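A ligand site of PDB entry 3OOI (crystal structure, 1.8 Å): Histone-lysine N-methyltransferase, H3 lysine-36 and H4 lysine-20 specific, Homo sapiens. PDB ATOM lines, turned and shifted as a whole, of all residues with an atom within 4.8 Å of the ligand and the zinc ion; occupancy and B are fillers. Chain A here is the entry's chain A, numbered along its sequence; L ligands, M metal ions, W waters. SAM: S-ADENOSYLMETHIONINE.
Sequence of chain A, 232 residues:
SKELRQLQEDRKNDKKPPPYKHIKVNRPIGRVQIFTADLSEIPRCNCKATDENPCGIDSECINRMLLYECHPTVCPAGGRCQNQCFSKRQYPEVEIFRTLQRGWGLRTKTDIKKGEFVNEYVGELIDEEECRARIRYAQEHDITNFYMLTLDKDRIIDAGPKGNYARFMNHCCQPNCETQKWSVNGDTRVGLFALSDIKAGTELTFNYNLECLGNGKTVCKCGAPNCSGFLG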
ATOM      1  N   GLN A 101     -13.495  13.939 -26.835  1.00  0.00           N
ATOM      2  CA  GLN A 101     -13.502  12.941 -27.892  1.00  0.00           C
ATOM      3  C   GLN A 101     -14.851  12.257 -28.087  1.00  0.00           C
ATOM      4  O   GLN A 101     -15.009  11.481 -29.023  1.00  0.00           O
ATOM      5  CB  GLN A 101     -12.458  11.860 -27.594  1.00  0.00           C
ATOM      6  CG  GLN A 101     -11.030  12.369 -27.570  1.00  0.00           C
ATOM      7  CD  GLN A 101     -10.086  11.254 -27.220  1.00  0.00           C
ATOM      8  OE1 GLN A 101      -9.859  10.954 -26.049  1.00  0.00           O
ATOM      9  NE2 GLN A 101      -9.543  10.611 -28.234  1.00  0.00           N
ATOM     10  N   ARG A 102     -15.787  12.526 -27.182  1.00  0.00           N
ATOM     11  CA  ARG A 102     -17.068  11.782 -27.134  1.00  0.00           C
ATOM     12  C   ARG A 102     -18.257  12.756 -27.123  1.00  0.00           C
ATOM     13  O   ARG A 102     -19.302  12.501 -26.498  1.00  0.00           O
ATOM     14  CB  ARG A 102     -17.078  10.834 -25.914  1.00  0.00           C
ATOM     15  CG  ARG A 102     -15.977   9.737 -25.983  1.00  0.00           C
ATOM     16  CD  ARG A 102     -15.734   9.022 -24.619  1.00  0.00           C
ATOM     17  NE  ARG A 102     -15.258   9.985 -23.633  1.00  0.00           N
ATOM     18  CZ  ARG A 102     -15.953  10.385 -22.577  1.00  0.00           C
ATOM     19  NH1 ARG A 102     -17.143   9.852 -22.308  1.00  0.00           N
ATOM     20  NH2 ARG A 102     -15.462  11.323 -21.759  1.00  0.00           N
ATOM     21  N   GLY A 103     -18.083  13.886 -27.789  1.00  0.00           N
ATOM     22  CA  GLY A 103     -19.146  14.902 -27.876  1.00  0.00           C
ATOM     23  C   GLY A 103     -19.632  15.381 -26.519  1.00  0.00           C
ATOM     24  O   GLY A 103     -18.823  15.614 -25.613  1.00  0.00           O
ATOM     25  N   TRP A 104     -20.956  15.543 -26.367  1.00  0.00           N
ATOM     26  CA  TRP A 104     -21.543  15.955 -25.078  1.00  0.00           C
ATOM     27  C   TRP A 104     -21.699  14.742 -24.190  1.00  0.00           C
ATOM     28  O   TRP A 104     -21.959  13.641 -24.683  1.00  0.00           O
ATOM     29  CB  TRP A 104     -22.902  16.676 -25.256  1.00  0.00           C
ATOM     30  CG  TRP A 104     -22.703  18.006 -25.948  1.00  0.00           C
ATOM     31  CD1 TRP A 104     -22.649  18.227 -27.285  1.00  0.00           C
ATOM     32  CD2 TRP A 104     -22.449  19.282 -25.316  1.00  0.00           C
ATOM     33  NE1 TRP A 104     -22.406  19.557 -27.539  1.00  0.00           N
ATOM     34  CE2 TRP A 104     -22.276  20.228 -26.350  1.00  0.00           C
ATOM     35  CE3 TRP A 104     -22.361  19.709 -23.988  1.00  0.00           C
ATOM     36  CZ2 TRP A 104     -22.013  21.579 -26.103  1.00  0.00           C
ATOM     37  CZ3 TRP A 104     -22.116  21.073 -23.740  1.00  0.00           C
ATOM     38  CH2 TRP A 104     -21.936  21.980 -24.792  1.00  0.00           C
ATOM     39  N   TYR A 121     -34.209   5.480 -19.831  1.00  0.00           N
ATOM     40  CA  TYR A 121     -33.873   5.829 -21.208  1.00  0.00           C
ATOM     41  C   TYR A 121     -35.166   6.020 -21.983  1.00  0.00           C
ATOM     42  O   TYR A 121     -35.839   5.051 -22.357  1.00  0.00           O
ATOM     43  CB  TYR A 121     -32.971   4.772 -21.840  1.00  0.00           C
ATOM     44  CG  TYR A 121     -32.260   5.281 -23.062  1.00  0.00           C
ATOM     45  CD1 TYR A 121     -31.019   5.912 -22.954  1.00  0.00           C
ATOM     46  CD2 TYR A 121     -32.830   5.129 -24.332  1.00  0.00           C
ATOM     47  CE1 TYR A 121     -30.357   6.409 -24.103  1.00  0.00           C
ATOM     48  CE2 TYR A 121     -32.171   5.605 -25.476  1.00  0.00           C
ATOM     49  CZ  TYR A 121     -30.942   6.242 -25.347  1.00  0.00           C
ATOM     50  OH  TYR A 121     -30.295   6.707 -26.484  1.00  0.00           O
ATOM     51  N   THR A 144     -22.792  11.047 -36.868  1.00  0.00           N
ATOM     52  CA  THR A 144     -22.165   9.889 -36.249  1.00  0.00           C
ATOM     53  C   THR A 144     -22.695   9.660 -34.830  1.00  0.00           C
ATOM     54  O   THR A 144     -22.219   8.773 -34.122  1.00  0.00           O
ATOM     55  CB  THR A 144     -20.627  10.060 -36.179  1.00  0.00           C
ATOM     56  OG1 THR A 144     -20.332  11.317 -35.566  1.00  0.00           O
ATOM     57  CG2 THR A 144     -20.015  10.033 -37.589  1.00  0.00           C
ATOM     58  N   ASN A 145     -23.670  10.475 -34.423  1.00  0.00           N
ATOM     59  CA  ASN A 145     -24.329  10.336 -33.126  1.00  0.00           C
ATOM     60  C   ASN A 145     -25.635   9.601 -33.296  1.00  0.00           C
ATOM     61  O   ASN A 145     -26.509  10.056 -34.034  1.00  0.00           O
ATOM     62  CB  ASN A 145     -24.649  11.698 -32.519  1.00  0.00           C
ATOM     63  CG  ASN A 145     -23.463  12.313 -31.814  1.00  0.00           C
ATOM     64  OD1 ASN A 145     -22.864  11.715 -30.925  1.00  0.00           O
ATOM     65  ND2 ASN A 145     -23.125  13.535 -32.212  1.00  0.00           N
ATOM     66  N   PHE A 146     -25.781   8.491 -32.591  1.00  0.00           N
ATOM     67  CA  PHE A 146     -27.006   7.699 -32.628  1.00  0.00           C
ATOM     68  C   PHE A 146     -27.497   7.541 -31.221  1.00  0.00           C
ATOM     69  O   PHE A 146     -26.690   7.499 -30.281  1.00  0.00           O
ATOM     70  CB  PHE A 146     -26.744   6.330 -33.275  1.00  0.00           C
ATOM     71  CG  PHE A 146     -26.309   6.425 -34.703  1.00  0.00           C
ATOM     72  CD1 PHE A 146     -27.249   6.566 -35.712  1.00  0.00           C
ATOM     73  CD2 PHE A 146     -24.948   6.433 -35.031  1.00  0.00           C
ATOM     74  CE1 PHE A 146     -26.840   6.686 -37.055  1.00  0.00           C
ATOM     75  CE2 PHE A 146     -24.529   6.562 -36.371  1.00  0.00           C
ATOM     76  CZ  PHE A 146     -25.482   6.682 -37.375  1.00  0.00           C
ATOM     77  N   TYR A 147     -28.809   7.443 -31.061  1.00  0.00           N
ATOM     78  CA  TYR A 147     -29.439   7.416 -29.726  1.00  0.00           C
ATOM     79  C   TYR A 147     -30.486   6.312 -29.672  1.00  0.00           C
ATOM     80  O   TYR A 147     -31.462   6.426 -28.930  1.00  0.00           O
ATOM     81  CB  TYR A 147     -30.142   8.760 -29.440  1.00  0.00           C
ATOM     82  CG  TYR A 147     -29.242   9.965 -29.522  1.00  0.00           C
ATOM     83  CD1 TYR A 147     -28.601  10.460 -28.387  1.00  0.00           C
ATOM     84  CD2 TYR A 147     -29.051  10.631 -30.738  1.00  0.00           C
ATOM     85  CE1 TYR A 147     -27.772  11.578 -28.466  1.00  0.00           C
ATOM     86  CE2 TYR A 147     -28.212  11.740 -30.827  1.00  0.00           C
ATOM     87  CZ  TYR A 147     -27.585  12.202 -29.680  1.00  0.00           C
ATOM     88  OH  TYR A 147     -26.757  13.296 -29.785  1.00  0.00           O
ATOM     89  N   ARG A 167     -30.019  10.463 -22.728  1.00  0.00           N
ATOM     90  CA  ARG A 167     -29.505  10.517 -24.093  1.00  0.00           C
ATOM     91  C   ARG A 167     -28.066  11.026 -24.160  1.00  0.00           C
ATOM     92  O   ARG A 167     -27.385  10.821 -25.166  1.00  0.00           O
ATOM     93  CB  ARG A 167     -30.407  11.399 -24.981  1.00  0.00           C
ATOM     94  CG  ARG A 167     -30.184  12.880 -24.793  1.00  0.00           C
ATOM     95  CD  ARG A 167     -31.265  13.726 -25.455  1.00  0.00           C
ATOM     96  NE  ARG A 167     -31.210  13.721 -26.932  1.00  0.00           N
ATOM     97  CZ  ARG A 167     -30.374  14.443 -27.681  1.00  0.00           C
ATOM     98  NH1 ARG A 167     -30.452  14.394 -29.000  1.00  0.00           N
ATOM     99  NH2 ARG A 167     -29.458  15.227 -27.119  1.00  0.00           N
ATOM    100  N   PHE A 168     -27.610  11.688 -23.106  1.00  0.00           N
ATOM    101  CA  PHE A 168     -26.259  12.225 -23.086  1.00  0.00           C
ATOM    102  C   PHE A 168     -25.224  11.303 -22.436  1.00  0.00           C
ATOM    103  O   PHE A 168     -24.019  11.650 -22.383  1.00  0.00           O
ATOM    104  CB  PHE A 168     -26.249  13.573 -22.357  1.00  0.00           C
ATOM    105  CG  PHE A 168     -26.905  14.686 -23.133  1.00  0.00           C
ATOM    106  CD1 PHE A 168     -28.197  15.133 -22.794  1.00  0.00           C
ATOM    107  CD2 PHE A 168     -26.231  15.294 -24.185  1.00  0.00           C
ATOM    108  CE1 PHE A 168     -28.804  16.163 -23.540  1.00  0.00           C
ATOM    109  CE2 PHE A 168     -26.828  16.351 -24.914  1.00  0.00           C
ATOM    110  CZ  PHE A 168     -28.111  16.777 -24.578  1.00  0.00           C
ATOM    111  N   MET A 169     -25.654  10.145 -21.964  1.00  0.00           N
ATOM    112  CA  MET A 169     -24.733   9.219 -21.299  1.00  0.00           C
ATOM    113  C   MET A 169     -23.893   8.435 -22.304  1.00  0.00           C
ATOM    114  O   MET A 169     -24.426   7.726 -23.162  1.00  0.00           O
ATOM    115  CB  MET A 169     -25.492   8.283 -20.359  1.00  0.00           C
ATOM    116  CG  MET A 169     -25.918   9.027 -19.103  1.00  0.00           C
ATOM    117  SD  MET A 169     -26.966   8.091 -18.004  1.00  0.00           S
ATOM    118  CE  MET A 169     -25.830   6.794 -17.462  1.00  0.00           C
ATOM    119  N   ASN A 170     -22.582   8.606 -22.192  1.00  0.00           N
ATOM    120  CA  ASN A 170     -21.622   7.987 -23.105  1.00  0.00           C
ATOM    121  C   ASN A 170     -21.332   6.538 -22.756  1.00  0.00           C
ATOM    122  O   ASN A 170     -21.610   6.087 -21.641  1.00  0.00           O
ATOM    123  CB  ASN A 170     -20.324   8.817 -23.133  1.00  0.00           C
ATOM    124  CG  ASN A 170     -20.471  10.087 -23.976  1.00  0.00           C
ATOM    125  OD1 ASN A 170     -20.000  11.162 -23.584  1.00  0.00           O
ATOM    126  ND2 ASN A 170     -21.133   9.963 -25.107  1.00  0.00           N
ATOM    127  N   HIS A 171     -20.753   5.816 -23.710  1.00  0.00           N
ATOM    128  CA  HIS A 171     -20.343   4.416 -23.489  1.00  0.00           C
ATOM    129  C   HIS A 171     -18.974   4.363 -22.808  1.00  0.00           C
ATOM    130  O   HIS A 171     -18.076   5.115 -23.162  1.00  0.00           O
ATOM    131  CB  HIS A 171     -20.233   3.656 -24.831  1.00  0.00           C
ATOM    132  CG  HIS A 171     -19.457   2.377 -24.692  1.00  0.00           C
ATOM    133  ND1 HIS A 171     -20.050   1.195 -24.328  1.00  0.00           N
ATOM    134  CD2 HIS A 171     -18.121   2.125 -24.768  1.00  0.00           C
ATOM    135  CE1 HIS A 171     -19.132   0.250 -24.224  1.00  0.00           C
ATOM    136  NE2 HIS A 171     -17.953   0.785 -24.494  1.00  0.00           N
ATOM    137  N   CYS A 173     -16.188   1.173 -21.372  1.00  0.00           N
ATOM    138  CA  CYS A 173     -15.841  -0.244 -21.143  1.00  0.00           C
ATOM    139  C   CYS A 173     -15.618  -0.554 -19.654  1.00  0.00           C
ATOM    140  O   CYS A 173     -15.663  -1.713 -19.277  1.00  0.00           O
ATOM    141  CB  CYS A 173     -14.621  -0.635 -21.984  1.00  0.00           C
ATOM    142  SG  CYS A 173     -14.922  -0.506 -23.789  1.00  0.00           S
ATOM    143  N   TYR A 208     -22.706   0.156 -23.531  1.00  0.00           N
ATOM    144  CA  TYR A 208     -23.751   0.079 -24.537  1.00  0.00           C
ATOM    145  C   TYR A 208     -24.045  -1.364 -24.962  1.00  0.00           C
ATOM    146  O   TYR A 208     -25.147  -1.644 -25.452  1.00  0.00           O
ATOM    147  CB  TYR A 208     -23.359   0.887 -25.778  1.00  0.00           C
ATOM    148  CG  TYR A 208     -23.458   2.402 -25.667  1.00  0.00           C
ATOM    149  CD1 TYR A 208     -23.669   3.051 -24.434  1.00  0.00           C
ATOM    150  CD2 TYR A 208     -23.291   3.197 -26.806  1.00  0.00           C
ATOM    151  CE1 TYR A 208     -23.737   4.457 -24.351  1.00  0.00           C
ATOM    152  CE2 TYR A 208     -23.339   4.583 -26.735  1.00  0.00           C
ATOM    153  CZ  TYR A 208     -23.582   5.215 -25.510  1.00  0.00           C
ATOM    154  OH  TYR A 208     -23.618   6.595 -25.460  1.00  0.00           O
ATOM    155  N   CYS A 212     -26.362   0.236 -29.229  1.00  0.00           N
ATOM    156  CA  CYS A 212     -26.653   1.568 -29.789  1.00  0.00           C
ATOM    157  C   CYS A 212     -26.656   1.454 -31.307  1.00  0.00           C
ATOM    158  O   CYS A 212     -25.593   1.409 -31.932  1.00  0.00           O
ATOM    159  CB  CYS A 212     -25.661   2.615 -29.285  1.00  0.00           C
ATOM    160  SG  CYS A 212     -26.157   4.334 -29.707  1.00  0.00           S
ATOM    161  N   ASN A 215     -23.930   2.297 -34.393  1.00  0.00           N
ATOM    162  CA  ASN A 215     -22.533   2.384 -33.937  1.00  0.00           C
ATOM    163  C   ASN A 215     -21.711   1.103 -34.040  1.00  0.00           C
ATOM    164  O   ASN A 215     -20.639   0.982 -33.402  1.00  0.00           O
ATOM    165  CB  ASN A 215     -22.485   2.924 -32.498  1.00  0.00           C
ATOM    166  CG  ASN A 215     -22.693   4.426 -32.424  1.00  0.00           C
ATOM    167  OD1 ASN A 215     -23.615   4.879 -31.746  1.00  0.00           O
ATOM    168  ND2 ASN A 215     -21.838   5.202 -33.097  1.00  0.00           N
ATOM    169  N   THR A 218     -18.129   1.759 -34.809  1.00  0.00           N
ATOM    170  CA  THR A 218     -17.501   2.890 -34.128  1.00  0.00           C
ATOM    171  C   THR A 218     -16.347   2.476 -33.222  1.00  0.00           C
ATOM    172  O   THR A 218     -16.443   1.495 -32.473  1.00  0.00           O
ATOM    173  CB  THR A 218     -18.568   3.701 -33.342  1.00  0.00           C
ATOM    174  OG1 THR A 218     -19.590   4.097 -34.266  1.00  0.00           O
ATOM    175  CG2 THR A 218     -17.945   4.942 -32.691  1.00  0.00           C
ATOM    176  N   VAL A 219     -15.246   3.230 -33.291  1.00  0.00           N
ATOM    177  CA  VAL A 219     -14.088   2.983 -32.442  1.00  0.00           C
ATOM    178  C   VAL A 219     -14.303   3.635 -31.085  1.00  0.00           C
ATOM    179  O   VAL A 219     -14.606   4.826 -31.007  1.00  0.00           O
ATOM    180  CB  VAL A 219     -12.769   3.524 -33.074  1.00  0.00           C
ATOM    181  CG1 VAL A 219     -11.595   3.362 -32.102  1.00  0.00           C
ATOM    182  CG2 VAL A 219     -12.474   2.798 -34.405  1.00  0.00           C
ATOM    183  N   CYS A 220     -14.126   2.859 -30.021  1.00  0.00           N
ATOM    184  CA  CYS A 220     -14.323   3.369 -28.682  1.00  0.00           C
ATOM    185  C   CYS A 220     -13.176   4.294 -28.245  1.00  0.00           C
ATOM    186  O   CYS A 220     -12.000   3.965 -28.421  1.00  0.00           O
ATOM    187  CB  CYS A 220     -14.452   2.233 -27.682  1.00  0.00           C
ATOM    188  SG  CYS A 220     -14.899   2.816 -26.019  1.00  0.00           S
ATOM    189  N   LYS A 221     -13.561   5.419 -27.655  1.00  0.00           N
ATOM    190  CA  LYS A 221     -12.598   6.394 -27.140  1.00  0.00           C
ATOM    191  C   LYS A 221     -12.733   6.541 -25.622  1.00  0.00           C
ATOM    192  O   LYS A 221     -12.376   7.577 -25.058  1.00  0.00           O
ATOM    193  CB  LYS A 221     -12.802   7.757 -27.826  1.00  0.00           C
ATOM    194  CG  LYS A 221     -12.722   7.733 -29.366  1.00  0.00           C
ATOM    195  CD  LYS A 221     -11.348   7.342 -29.848  1.00  0.00           C
ATOM    196  CE  LYS A 221     -11.327   7.174 -31.364  1.00  0.00           C
ATOM    197  NZ  LYS A 221     -10.009   6.617 -31.775  1.00  0.00           N
ATOM    198  N   CYS A 222     -13.222   5.490 -24.960  1.00  0.00           N
ATOM    199  CA  CYS A 222     -13.458   5.575 -23.499  1.00  0.00           C
ATOM    200  C   CYS A 222     -12.193   5.660 -22.658  1.00  0.00           C
ATOM    201  O   CYS A 222     -12.243   6.120 -21.516  1.00  0.00           O
ATOM    202  CB  CYS A 222     -14.345   4.438 -22.988  1.00  0.00           C
ATOM    203  SG  CYS A 222     -13.471   2.859 -22.653  1.00  0.00           S
ATOM    204  N   GLY A 223     -11.070   5.205 -23.217  1.00  0.00           N
ATOM    205  CA  GLY A 223      -9.766   5.303 -22.544  1.00  0.00           C
ATOM    206  C   GLY A 223      -9.518   4.346 -21.385  1.00  0.00           C
ATOM    207  O   GLY A 223      -8.473   4.450 -20.734  1.00  0.00           O
ATOM    208  N   CYS A 227     -10.290  -1.487 -22.502  1.00  0.00           N
ATOM    209  CA  CYS A 227     -11.148  -1.081 -23.629  1.00  0.00           C
ATOM    210  C   CYS A 227     -11.220  -2.158 -24.721  1.00  0.00           C
ATOM    211  O   CYS A 227     -10.190  -2.642 -25.206  1.00  0.00           O
ATOM    212  CB  CYS A 227     -10.707   0.246 -24.219  1.00  0.00           C
ATOM    213  SG  CYS A 227     -11.754   0.850 -25.555  1.00  0.00           S
ATOM    214  N   SER A 228     -12.442  -2.512 -25.108  1.00  0.00           N
ATOM    215  CA  SER A 228     -12.661  -3.510 -26.172  1.00  0.00           C
ATOM    216  C   SER A 228     -12.342  -2.952 -27.558  1.00  0.00           C
ATOM    217  O   SER A 228     -12.153  -3.722 -28.510  1.00  0.00           O
ATOM    218  CB  SER A 228     -14.132  -3.919 -26.170  1.00  0.00           C
ATOM    219  OG  SER A 228     -14.904  -2.816 -26.624  1.00  0.00           O
ATOM    220  N   GLY A 229     -12.336  -1.630 -27.679  1.00  0.00           N
ATOM    221  CA  GLY A 229     -12.147  -0.959 -28.966  1.00  0.00           C
ATOM    222  C   GLY A 229     -13.439  -0.615 -29.688  1.00  0.00           C
ATOM    223  O   GLY A 229     -13.438   0.039 -30.735  1.00  0.00           O
ATOM    224  N   PHE A 230     -14.561  -1.086 -29.129  1.00  0.00           N
ATOM    225  CA  PHE A 230     -15.877  -0.841 -29.721  1.00  0.00           C
ATOM    226  C   PHE A 230     -16.905  -0.491 -28.636  1.00  0.00           C
ATOM    227  O   PHE A 230     -16.598  -0.589 -27.433  1.00  0.00           O
ATOM    228  CB  PHE A 230     -16.320  -2.029 -30.586  1.00  0.00           C
ATOM    229  CG  PHE A 230     -16.289  -3.372 -29.877  1.00  0.00           C
ATOM    230  CD1 PHE A 230     -17.397  -3.820 -29.146  1.00  0.00           C
ATOM    231  CD2 PHE A 230     -15.186  -4.221 -29.996  1.00  0.00           C
ATOM    232  CE1 PHE A 230     -17.389  -5.082 -28.515  1.00  0.00           C
ATOM    233  CE2 PHE A 230     -15.168  -5.474 -29.363  1.00  0.00           C
ATOM    234  CZ  PHE A 230     -16.284  -5.911 -28.631  1.00  0.00           C
ATOM    235  N   LEU A 231     -18.101  -0.072 -29.042  1.00  0.00           N
ATOM    236  CA  LEU A 231     -19.088   0.377 -28.044  1.00  0.00           C
ATOM    237  C   LEU A 231     -19.856  -0.808 -27.457  1.00  0.00           C
ATOM    238  O   LEU A 231     -21.076  -0.917 -27.606  1.00  0.00           O
ATOM    239  CB  LEU A 231     -20.021   1.468 -28.614  1.00  0.00           C
ATOM    240  CG  LEU A 231     -19.355   2.701 -29.236  1.00  0.00           C
ATOM    241  CD1 LEU A 231     -20.423   3.810 -29.469  1.00  0.00           C
ATOM    242  CD2 LEU A 231     -18.164   3.231 -28.475  1.00  0.00           C
HETATM  243  N   SAM L   1     -21.904  11.951 -27.043  1.00  0.00           N
HETATM  244  CA  SAM L   1     -23.367  12.053 -27.354  1.00  0.00           C
HETATM  245  C   SAM L   1     -23.733  13.482 -27.769  1.00  0.00           C
HETATM  246  O   SAM L   1     -22.871  14.360 -28.028  1.00  0.00           O
HETATM  247  OXT SAM L   1     -24.913  13.790 -27.866  1.00  0.00           O
HETATM  248  CB  SAM L   1     -24.207  11.515 -26.185  1.00  0.00           C
HETATM  249  CG  SAM L   1     -24.264   9.969 -26.190  1.00  0.00           C
HETATM  250  SD  SAM L   1     -25.247   9.338 -27.594  1.00  0.00           S
HETATM  251  CE  SAM L   1     -26.406   8.194 -26.811  1.00  0.00           C
HETATM  252  C5' SAM L   1     -24.157   8.117 -28.350  1.00  0.00           C
HETATM  253  C4' SAM L   1     -23.087   8.692 -29.265  1.00  0.00           C
HETATM  254  O4' SAM L   1     -21.999   9.260 -28.541  1.00  0.00           O
HETATM  255  C3' SAM L   1     -22.509   7.599 -30.122  1.00  0.00           C
HETATM  256  O3' SAM L   1     -23.264   7.412 -31.299  1.00  0.00           O
HETATM  257  C2' SAM L   1     -21.096   8.076 -30.364  1.00  0.00           C
HETATM  258  O2' SAM L   1     -21.061   9.004 -31.451  1.00  0.00           O
HETATM  259  C1' SAM L   1     -20.763   8.834 -29.089  1.00  0.00           C
HETATM  260  N9  SAM L   1     -20.060   7.997 -28.094  1.00  0.00           N
HETATM  261  C8  SAM L   1     -20.544   7.631 -26.864  1.00  0.00           C
HETATM  262  N7  SAM L   1     -19.600   6.902 -26.216  1.00  0.00           N
HETATM  263  C5  SAM L   1     -18.510   6.835 -27.027  1.00  0.00           C
HETATM  264  C6  SAM L   1     -17.258   6.237 -26.858  1.00  0.00           C
HETATM  265  N6  SAM L   1     -16.942   5.556 -25.766  1.00  0.00           N
HETATM  266  N1  SAM L   1     -16.342   6.331 -27.863  1.00  0.00           N
HETATM  267  C2  SAM L   1     -16.629   7.025 -29.021  1.00  0.00           C
HETATM  268  N3  SAM L   1     -17.859   7.632 -29.195  1.00  0.00           N
HETATM  269  C4  SAM L   1     -18.775   7.538 -28.190  1.00  0.00           C
HETATM  270 ZN    ZN M   1     -13.767   1.490 -24.516  1.00  0.00          ZN
HETATM  271  O   HOH W   1     -27.148   7.373 -23.897  1.00  0.00           O
HETATM  272  O   HOH W   2     -19.775  11.163 -33.054  1.00  0.00           O
HETATM  273  O   HOH W   3     -17.659   8.672 -31.824  1.00  0.00           O
HETATM  274  O   HOH W   4     -25.552  16.266 -28.538  1.00  0.00           O
HETATM  275  O   HOH W   5     -20.656  12.237 -29.644  1.00  0.00           O
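The backbone NH (N) of Lys 221 sits at hydrogen-bond distance from a nitrogen (N1) of the ligand (2.9 Å). OD1 of Asn 215 is in hydrogen-bond range of O3' of the ligand (2.6 Å). The side-chain amide oxygen (OD1) of Asn 145 lies within hydrogen-bond range of an oxygen (O2') of the ligand (3.3 Å). OH of Tyr 147 lies within hydrogen-bond range of OXT of the ligand (2.7 Å). ND2 of Asn 170 lies close to N of the ligand, at 2.9 Å. N of His 171 is in hydrogen-bond range of N7 of the ligand (3.0 Å). The side-chain sulfur (SG) of Cys 220 lies close to a nitrogen (N6) of the ligand, at 3.4 Å. O of His 171 lies within hydrogen-bond range of N6 of the ligand. The backbone NH (N) of Trp 104 is in hydrogen-bond range of an oxygen (O) of the ligand (2.8 Å). The backbone carbonyl oxygen (O) of Thr 144 is in hydrogen-bond range of an oxygen (O2') of the ligand (2.9 Å). O3' of the ligand is in hydrogen-bond range of N of Phe 146, at 3.0 Å. The backbone carbonyl oxygen of Trp 104 sits at hydrogen-bond distance from a nitrogen (N) of the ligand (2.9 Å). A nitrogen (N) of the ligand lies within hydrogen-bond range of the backbone carbonyl oxygen (O) of Arg 102 (2.7 Å).
OG1 of Thr 218 sits at hydrogen-bond distance from ND2 of Asn 215. The backbone NH (N) of Tyr 208 is in hydrogen-bond range of a ring nitrogen (ND1) of His 171, 3.0 Å away. The backbone carbonyl oxygen (O) of Tyr 147 sits at hydrogen-bond distance from the side-chain hydroxyl (OH) of Tyr 121, 2.7 Å away. The side-chain amide oxygen (OD1) of Asn 170 sits close to the backbone carbonyl oxygen (O) of Trp 104, at 3.3 Å. The side-chain sulfur (SG) of Cys 212 sits at hydrogen-bond distance from the backbone carbonyl oxygen (O) of Phe 146, 3.3 Å away. The backbone NH of Cys 220 sits at hydrogen-bond distance from the backbone carbonyl oxygen of Gly 229. A ring nitrogen (NE2) of His 171 lies close to the side-chain sulfur of Cys 173. SG of Cys 227 lies close to N of Gly 229 (3.3 Å).
SD of the ligand sits close to O of Arg 167 (3.6 Å). C of Gly 103 touches O of the ligand (3.7 Å). Phe 168 touches the ligand. Met 169 touches the ligand. Tyr 208 touches the ligand (OH to C5', 3.3 Å). O of Val 219 touches C2 of the ligand (3.6 Å). Leu 231 touches the ligand. Hydrophobic or aromatic side chains that line the ligand: Trp 104, Tyr 147, His 171, Tyr 208 and Leu 231. Within 4 Å of the ligand: Arg 102, Gly 103, Trp 104, Thr 144, Asn 145, Phe 146, Tyr 147, Arg 167, Phe 168, Met 169, Asn 170, His 171, Tyr 208, Asn 215, Val 219, Cys 220, Lys 221, Cys 222 and Leu 231. The nearest printed residue that does not touch the ligand is Tyr 121 (4.2 Å).
Four residues have an atom within 4 Å of the zinc ion: Cys 173, Cys 220, Cys 222 and Cys 227.
The zinc ion is bound by the side-chain sulfur of Cys 220 (2.3 Å), the side-chain sulfur of Cys 222 (2.3 Å), the side-chain sulfur of Cys 227 (2.4 Å) and the side-chain sulfur of Cys 173 (2.4 Å). The zinc ion has four donor atoms within binding distance.
Water W4 lies within hydrogen-bond range of an oxygen (OXT) of the ligand (2.6 Å) and the side-chain hydroxyl (OH) of Tyr 147 (3.4 Å). Water W5 lies within hydrogen-bond range of the side-chain amide oxygen (OD1) of Asn 145, a nitrogen (N) of the ligand and the backbone carbonyl oxygen (O) of Arg 102. Water W2 bridges OG1 of Thr 144 (2.6 Å) and O2' of the ligand (3.0 Å).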
